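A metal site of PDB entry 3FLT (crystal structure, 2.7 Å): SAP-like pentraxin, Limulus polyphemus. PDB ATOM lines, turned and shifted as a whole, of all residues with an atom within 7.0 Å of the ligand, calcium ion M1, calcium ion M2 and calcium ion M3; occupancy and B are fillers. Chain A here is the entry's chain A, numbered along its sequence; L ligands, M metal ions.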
ATOM      1  N   THR A  47     -27.126  -8.779  15.458  1.00  0.00           N
ATOM      2  CA  THR A  47     -26.263  -8.524  14.314  1.00  0.00           C
ATOM      3  C   THR A  47     -25.301  -7.381  14.499  1.00  0.00           C
ATOM      4  O   THR A  47     -25.665  -6.308  14.993  1.00  0.00           O
ATOM      5  CB  THR A  47     -27.111  -8.239  13.052  1.00  0.00           C
ATOM      6  OG1 THR A  47     -27.809  -9.433  12.667  1.00  0.00           O
ATOM      7  CG2 THR A  47     -26.246  -7.792  11.886  1.00  0.00           C
ATOM      8  N   TYR A  49     -21.563  -5.671  12.497  1.00  0.00           N
ATOM      9  CA  TYR A  49     -20.614  -5.739  11.391  1.00  0.00           C
ATOM     10  C   TYR A  49     -19.206  -5.654  11.936  1.00  0.00           C
ATOM     11  O   TYR A  49     -18.875  -4.729  12.690  1.00  0.00           O
ATOM     12  CB  TYR A  49     -20.874  -4.619  10.376  1.00  0.00           C
ATOM     13  CG  TYR A  49     -22.177  -4.803   9.649  1.00  0.00           C
ATOM     14  CD1 TYR A  49     -23.350  -4.177  10.100  1.00  0.00           C
ATOM     15  CD2 TYR A  49     -22.278  -5.669   8.562  1.00  0.00           C
ATOM     16  CE1 TYR A  49     -24.578  -4.425   9.489  1.00  0.00           C
ATOM     17  CE2 TYR A  49     -23.489  -5.920   7.951  1.00  0.00           C
ATOM     18  CZ  TYR A  49     -24.638  -5.292   8.418  1.00  0.00           C
ATOM     19  OH  TYR A  49     -25.835  -5.577   7.829  1.00  0.00           O
ATOM     20  N   SER A  52     -15.565  -3.990   7.611  1.00  0.00           N
ATOM     21  CA  SER A  52     -16.272  -3.142   6.649  1.00  0.00           C
ATOM     22  C   SER A  52     -15.301  -2.500   5.665  1.00  0.00           C
ATOM     23  O   SER A  52     -14.337  -1.838   6.069  1.00  0.00           O
ATOM     24  CB  SER A  52     -17.033  -2.042   7.392  1.00  0.00           C
ATOM     25  OG  SER A  52     -17.455  -1.009   6.521  1.00  0.00           O
ATOM     26  N   ALA A  54     -15.079   0.004   2.222  1.00  0.00           N
ATOM     27  CA  ALA A  54     -15.788   0.949   1.376  1.00  0.00           C
ATOM     28  C   ALA A  54     -14.897   1.777   0.471  1.00  0.00           C
ATOM     29  O   ALA A  54     -13.759   2.090   0.796  1.00  0.00           O
ATOM     30  CB  ALA A  54     -16.622   1.879   2.245  1.00  0.00           C
ATOM     31  N   GLN A  58     -18.810   3.038  -3.655  1.00  0.00           N
ATOM     32  CA  GLN A  58     -19.560   1.959  -3.011  1.00  0.00           C
ATOM     33  C   GLN A  58     -19.126   1.770  -1.562  1.00  0.00           C
ATOM     34  O   GLN A  58     -18.039   1.281  -1.299  1.00  0.00           O
ATOM     35  CB  GLN A  58     -19.341   0.654  -3.789  1.00  0.00           C
ATOM     36  CG  GLN A  58     -19.938  -0.591  -3.156  1.00  0.00           C
ATOM     37  CD  GLN A  58     -21.457  -0.525  -3.030  1.00  0.00           C
ATOM     38  OE1 GLN A  58     -21.982   0.152  -2.139  1.00  0.00           O
ATOM     39  NE2 GLN A  58     -22.162  -1.219  -3.924  1.00  0.00           N
ATOM     40  N   ASP A  59     -19.996   2.154  -0.627  1.00  0.00           N
ATOM     41  CA  ASP A  59     -19.688   2.031   0.796  1.00  0.00           C
ATOM     42  C   ASP A  59     -19.867   0.589   1.303  1.00  0.00           C
ATOM     43  O   ASP A  59     -19.397   0.244   2.388  1.00  0.00           O
ATOM     44  CB  ASP A  59     -20.576   2.997   1.598  1.00  0.00           C
ATOM     45  CG  ASP A  59     -22.062   2.743   1.405  1.00  0.00           C
ATOM     46  OD1 ASP A  59     -22.539   2.805   0.248  1.00  0.00           O
ATOM     47  OD2 ASP A  59     -22.753   2.461   2.408  1.00  0.00           O
ATOM     48  N   ASN A  60     -20.532  -0.248   0.513  1.00  0.00           N
ATOM     49  CA  ASN A  60     -20.739  -1.632   0.886  1.00  0.00           C
ATOM     50  C   ASN A  60     -20.010  -2.574  -0.066  1.00  0.00           C
ATOM     51  O   ASN A  60     -20.622  -3.456  -0.670  1.00  0.00           O
ATOM     52  CB  ASN A  60     -22.237  -1.979   0.881  1.00  0.00           C
ATOM     53  CG  ASN A  60     -23.013  -1.267   1.979  1.00  0.00           C
ATOM     54  OD1 ASN A  60     -22.547  -0.280   2.544  1.00  0.00           O
ATOM     55  ND2 ASN A  60     -24.205  -1.770   2.283  1.00  0.00           N
ATOM     56  N   ILE A  63     -18.559  -6.527   3.487  1.00  0.00           N
ATOM     57  CA  ILE A  63     -18.887  -6.396   4.904  1.00  0.00           C
ATOM     58  C   ILE A  63     -19.198  -7.735   5.556  1.00  0.00           C
ATOM     59  O   ILE A  63     -20.087  -8.445   5.112  1.00  0.00           O
ATOM     60  CB  ILE A  63     -20.135  -5.519   5.132  1.00  0.00           C
ATOM     61  CG1 ILE A  63     -20.431  -4.694   3.873  1.00  0.00           C
ATOM     62  CG2 ILE A  63     -19.917  -4.630   6.346  1.00  0.00           C
ATOM     63  CD1 ILE A  63     -21.746  -3.909   3.960  1.00  0.00           C
ATOM     64  N   GLN A  79     -21.667  -9.569   2.777  1.00  0.00           N
ATOM     65  CA  GLN A  79     -22.340  -8.727   1.816  1.00  0.00           C
ATOM     66  C   GLN A  79     -21.299  -8.193   0.846  1.00  0.00           C
ATOM     67  O   GLN A  79     -20.286  -7.648   1.271  1.00  0.00           O
ATOM     68  CB  GLN A  79     -23.061  -7.563   2.513  1.00  0.00           C
ATOM     69  CG  GLN A  79     -23.728  -6.593   1.536  1.00  0.00           C
ATOM     70  CD  GLN A  79     -24.452  -5.441   2.225  1.00  0.00           C
ATOM     71  OE1 GLN A  79     -24.734  -4.420   1.610  1.00  0.00           O
ATOM     72  NE2 GLN A  79     -24.756  -5.607   3.515  1.00  0.00           N
ATOM     73  N   SER A  83     -25.031  -6.208  -1.930  1.00  0.00           N
ATOM     74  CA  SER A  83     -26.037  -7.247  -2.093  1.00  0.00           C
ATOM     75  C   SER A  83     -26.715  -7.350  -0.737  1.00  0.00           C
ATOM     76  O   SER A  83     -26.439  -6.557   0.159  1.00  0.00           O
ATOM     77  CB  SER A  83     -25.383  -8.590  -2.452  1.00  0.00           C
ATOM     78  OG  SER A  83     -24.605  -9.095  -1.369  1.00  0.00           O
ATOM     79  N   ASN A  85     -27.335  -9.208   2.880  1.00  0.00           N
ATOM     80  CA  ASN A  85     -26.457 -10.010   3.719  1.00  0.00           C
ATOM     81  C   ASN A  85     -26.801 -11.480   3.565  1.00  0.00           C
ATOM     82  O   ASN A  85     -27.943 -11.881   3.775  1.00  0.00           O
ATOM     83  CB  ASN A  85     -26.570  -9.597   5.177  1.00  0.00           C
ATOM     84  CG  ASN A  85     -25.984  -8.240   5.433  1.00  0.00           C
ATOM     85  OD1 ASN A  85     -24.814  -7.996   5.141  1.00  0.00           O
ATOM     86  ND2 ASN A  85     -26.787  -7.344   5.976  1.00  0.00           N
ATOM     87  N   GLU A 145     -20.003  -0.127  10.746  1.00  0.00           N
ATOM     88  CA  GLU A 145     -20.361  -0.278   9.327  1.00  0.00           C
ATOM     89  C   GLU A 145     -20.373   1.092   8.644  1.00  0.00           C
ATOM     90  O   GLU A 145     -21.177   1.963   8.974  1.00  0.00           O
ATOM     91  CB  GLU A 145     -21.745  -0.934   9.212  1.00  0.00           C
ATOM     92  CG  GLU A 145     -22.029  -1.637   7.901  1.00  0.00           C
ATOM     93  CD  GLU A 145     -22.198  -0.677   6.723  1.00  0.00           C
ATOM     94  OE1 GLU A 145     -23.033   0.248   6.833  1.00  0.00           O
ATOM     95  OE2 GLU A 145     -21.508  -0.854   5.692  1.00  0.00           O
ATOM     96  N   GLN A 146     -19.475   1.276   7.678  1.00  0.00           N
ATOM     97  CA  GLN A 146     -19.359   2.552   6.971  1.00  0.00           C
ATOM     98  C   GLN A 146     -20.474   2.839   5.984  1.00  0.00           C
ATOM     99  O   GLN A 146     -20.881   1.969   5.221  1.00  0.00           O
ATOM    100  CB  GLN A 146     -18.043   2.603   6.193  1.00  0.00           C
ATOM    101  CG  GLN A 146     -16.793   2.378   6.990  1.00  0.00           C
ATOM    102  CD  GLN A 146     -15.582   2.227   6.094  1.00  0.00           C
ATOM    103  OE1 GLN A 146     -15.015   3.210   5.615  1.00  0.00           O
ATOM    104  NE2 GLN A 146     -15.183   0.990   5.845  1.00  0.00           N
ATOM    105  N   ASP A 147     -20.950   4.078   5.988  1.00  0.00           N
ATOM    106  CA  ASP A 147     -21.962   4.517   5.026  1.00  0.00           C
ATOM    107  C   ASP A 147     -21.255   5.611   4.253  1.00  0.00           C
ATOM    108  O   ASP A 147     -21.813   6.243   3.371  1.00  0.00           O
ATOM    109  CB  ASP A 147     -23.197   5.071   5.713  1.00  0.00           C
ATOM    110  CG  ASP A 147     -24.075   3.990   6.293  1.00  0.00           C
ATOM    111  OD1 ASP A 147     -24.275   2.974   5.615  1.00  0.00           O
ATOM    112  OD2 ASP A 147     -24.571   4.153   7.419  1.00  0.00           O
ATOM    113  N   LYS A 148     -19.998   5.804   4.610  1.00  0.00           N
ATOM    114  CA  LYS A 148     -19.130   6.808   4.020  1.00  0.00           C
ATOM    115  C   LYS A 148     -17.690   6.412   4.376  1.00  0.00           C
ATOM    116  O   LYS A 148     -17.456   5.766   5.404  1.00  0.00           O
ATOM    117  CB  LYS A 148     -19.465   8.167   4.616  1.00  0.00           C
ATOM    118  CG  LYS A 148     -18.520   9.246   4.231  1.00  0.00           C
ATOM    119  CD  LYS A 148     -18.941  10.547   4.863  1.00  0.00           C
ATOM    120  CE  LYS A 148     -18.934  10.467   6.363  1.00  0.00           C
ATOM    121  NZ  LYS A 148     -19.128  11.820   6.952  1.00  0.00           N
ATOM    122  N   GLY A 151     -16.617   6.537   7.965  1.00  0.00           N
ATOM    123  CA  GLY A 151     -17.648   7.107   8.805  1.00  0.00           C
ATOM    124  C   GLY A 151     -19.093   6.745   8.476  1.00  0.00           C
ATOM    125  O   GLY A 151     -19.362   5.744   7.809  1.00  0.00           O
ATOM    126  N   GLY A 152     -20.013   7.581   8.961  1.00  0.00           N
ATOM    127  CA  GLY A 152     -21.425   7.337   8.744  1.00  0.00           C
ATOM    128  C   GLY A 152     -21.846   6.082   9.471  1.00  0.00           C
ATOM    129  O   GLY A 152     -22.588   5.264   8.925  1.00  0.00           O
ATOM    130  N   PHE A 153     -21.395   5.923  10.709  1.00  0.00           N
ATOM    131  CA  PHE A 153     -21.719   4.736  11.485  1.00  0.00           C
ATOM    132  C   PHE A 153     -23.117   4.760  12.105  1.00  0.00           C
ATOM    133  O   PHE A 153     -23.624   5.824  12.442  1.00  0.00           O
ATOM    134  CB  PHE A 153     -20.687   4.529  12.597  1.00  0.00           C
ATOM    135  CG  PHE A 153     -19.251   4.571  12.115  1.00  0.00           C
ATOM    136  CD1 PHE A 153     -18.845   3.820  11.003  1.00  0.00           C
ATOM    137  CD2 PHE A 153     -18.300   5.341  12.791  1.00  0.00           C
ATOM    138  CE1 PHE A 153     -17.509   3.831  10.586  1.00  0.00           C
ATOM    139  CE2 PHE A 153     -16.964   5.352  12.374  1.00  0.00           C
ATOM    140  CZ  PHE A 153     -16.570   4.599  11.268  1.00  0.00           C
ATOM    141  N   GLU A 154     -23.710   3.584  12.230  1.00  0.00           N
ATOM    142  CA  GLU A 154     -25.038   3.413  12.827  1.00  0.00           C
ATOM    143  C   GLU A 154     -24.872   2.498  14.041  1.00  0.00           C
ATOM    144  O   GLU A 154     -24.275   1.434  13.929  1.00  0.00           O
ATOM    145  CB  GLU A 154     -25.995   2.784  11.815  1.00  0.00           C
ATOM    146  CG  GLU A 154     -25.961   3.448  10.455  1.00  0.00           C
ATOM    147  CD  GLU A 154     -27.205   3.162   9.629  1.00  0.00           C
ATOM    148  OE1 GLU A 154     -28.312   3.504  10.104  1.00  0.00           O
ATOM    149  OE2 GLU A 154     -27.097   2.590   8.527  1.00  0.00           O
ATOM    150  N   GLN A 156     -26.960   0.522  15.713  1.00  0.00           N
ATOM    151  CA  GLN A 156     -27.543  -0.810  15.628  1.00  0.00           C
ATOM    152  C   GLN A 156     -26.813  -1.723  14.670  1.00  0.00           C
ATOM    153  O   GLN A 156     -27.178  -2.887  14.524  1.00  0.00           O
ATOM    154  CB  GLN A 156     -29.043  -0.754  15.302  1.00  0.00           C
ATOM    155  CG  GLN A 156     -29.465  -0.563  13.846  1.00  0.00           C
ATOM    156  CD  GLN A 156     -29.040   0.765  13.243  1.00  0.00           C
ATOM    157  OE1 GLN A 156     -28.880   1.764  13.947  1.00  0.00           O
ATOM    158  NE2 GLN A 156     -28.863   0.777  11.928  1.00  0.00           N
ATOM    159  N   GLU A 157     -25.770  -1.190  14.019  1.00  0.00           N
ATOM    160  CA  GLU A 157     -24.981  -1.991  13.081  1.00  0.00           C
ATOM    161  C   GLU A 157     -23.553  -2.205  13.569  1.00  0.00           C
ATOM    162  O   GLU A 157     -22.746  -2.841  12.900  1.00  0.00           O
ATOM    163  CB  GLU A 157     -24.950  -1.321  11.700  1.00  0.00           C
ATOM    164  CG  GLU A 157     -26.318  -1.016  11.133  1.00  0.00           C
ATOM    165  CD  GLU A 157     -26.291  -0.648   9.664  1.00  0.00           C
ATOM    166  OE1 GLU A 157     -25.562   0.283   9.270  1.00  0.00           O
ATOM    167  OE2 GLU A 157     -27.011  -1.306   8.877  1.00  0.00           O
HETATM  168  C1  LIG L   1     -26.148  -1.801   5.430  1.00  0.00           C
HETATM  169  C2  LIG L   1     -26.643  -3.263   5.388  1.00  0.00           C
HETATM  170  O1  LIG L   1     -26.374   1.008   6.294  1.00  0.00           O
HETATM  171  O2  LIG L   1     -25.064   0.542   4.190  1.00  0.00           O
HETATM  172  O3  LIG L   1     -27.332   1.573   3.915  1.00  0.00           O
HETATM  173  O4  LIG L   1     -27.028  -0.943   4.664  1.00  0.00           O
HETATM  174  N1  LIG L   1     -27.160  -3.649   6.738  1.00  0.00           N
HETATM  175  P1  LIG L   1     -26.423   0.543   4.755  1.00  0.00           P
HETATM  176 CA    CA M   1     -24.686   1.677   7.701  1.00  0.00          CA
HETATM  177 CA    CA M   2     -22.683   1.048   4.545  1.00  0.00          CA
HETATM  178 CA    CA M   3     -28.587   1.079   7.602  1.00  0.00          CA
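OH of Tyr 49 is in hydrogen-bond range of N1 of the ligand (2.6 Å).
Calcium ion M1 is bound by the side-chain carboxylate (OE1) of Glu 157 (2.3 Å), an oxygen (O1) of the ligand (2.3 Å), the side-chain carboxylate (OE1) of Glu 145 (2.4 Å), the side-chain carboxylate (OD1) of Asp 147 (2.5 Å), the side-chain carboxylate (OD2) of Asp 147 (2.5 Å) and the side-chain carboxylate (OE2) of Glu 154 (2.7 Å).
Of the 21 residues printed, 2 come within 4 Å of calcium ion M3.
Calcium ion M2 is bound by O of Gln 146, OD1 of Asn 60, OE1 of Glu 145, O2 of the ligand, OE2 of Glu 145, OD2 of Asp 59 and OD1 of Asp 147.
Within 4 Å of calcium ion M1: Glu 145, Asp 147, Glu 154 and Glu 157.
Within 4 Å of calcium ion M2: Asp 59, Asn 60, Glu 145, Gln 146 and Asp 147. The nearest printed residue that does not touch calcium ion M2 is Ile 63 (5.1 Å).
Residues that only touch the ligand: Gln 79 (3.5 Å) and Asn 85 (3.8 Å). Hydrophobic or aromatic side chains within 4 Å of the ligand: Tyr 49. Nine residues have an atom within 4 Å of the ligand: Tyr 49, Asp 59, Asn 60, Gln 79, Asn 85, Glu 145, Asp 147, Glu 154 and Glu 157.
Calcium ion M3 is bound by OE2 of Glu 154 (2.3 Å) and O1 of the ligand (2.6 Å). Slightly farther from calcium ion M3 lies the side-chain carboxylate (OE2) of Glu 157 (3.1 Å).
N of Ile 63 lies within hydrogen-bond range of O of Gln 79 (3.0 Å). The side-chain amide oxygen (OE1) of Gln 79 lies close to the backbone carbonyl oxygen (O) of Ser 83, at 3.1 Å. OH of Tyr 49 is in hydrogen-bond range of ND2 of Asn 85 (2.7 Å). The side-chain amide nitrogen (ND2) of Asn 60 is in hydrogen-bond range of the side-chain amide oxygen (OE1) of Gln 79 (2.8 Å). The backbone carbonyl oxygen (O) of Glu 157 is in hydrogen-bond range of the backbone NH (N) of Tyr 49 (3.1 Å). NE2 of Gln 146 lies within hydrogen-bond range of O of Ser 52, 3.0 Å away. OD1 of Asn 85 is in hydrogen-bond range of NE2 of Gln 79, at 2.9 Å. OE1 of Glu 154 sits at hydrogen-bond distance from NE2 of Gln 156 (3.3 Å).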
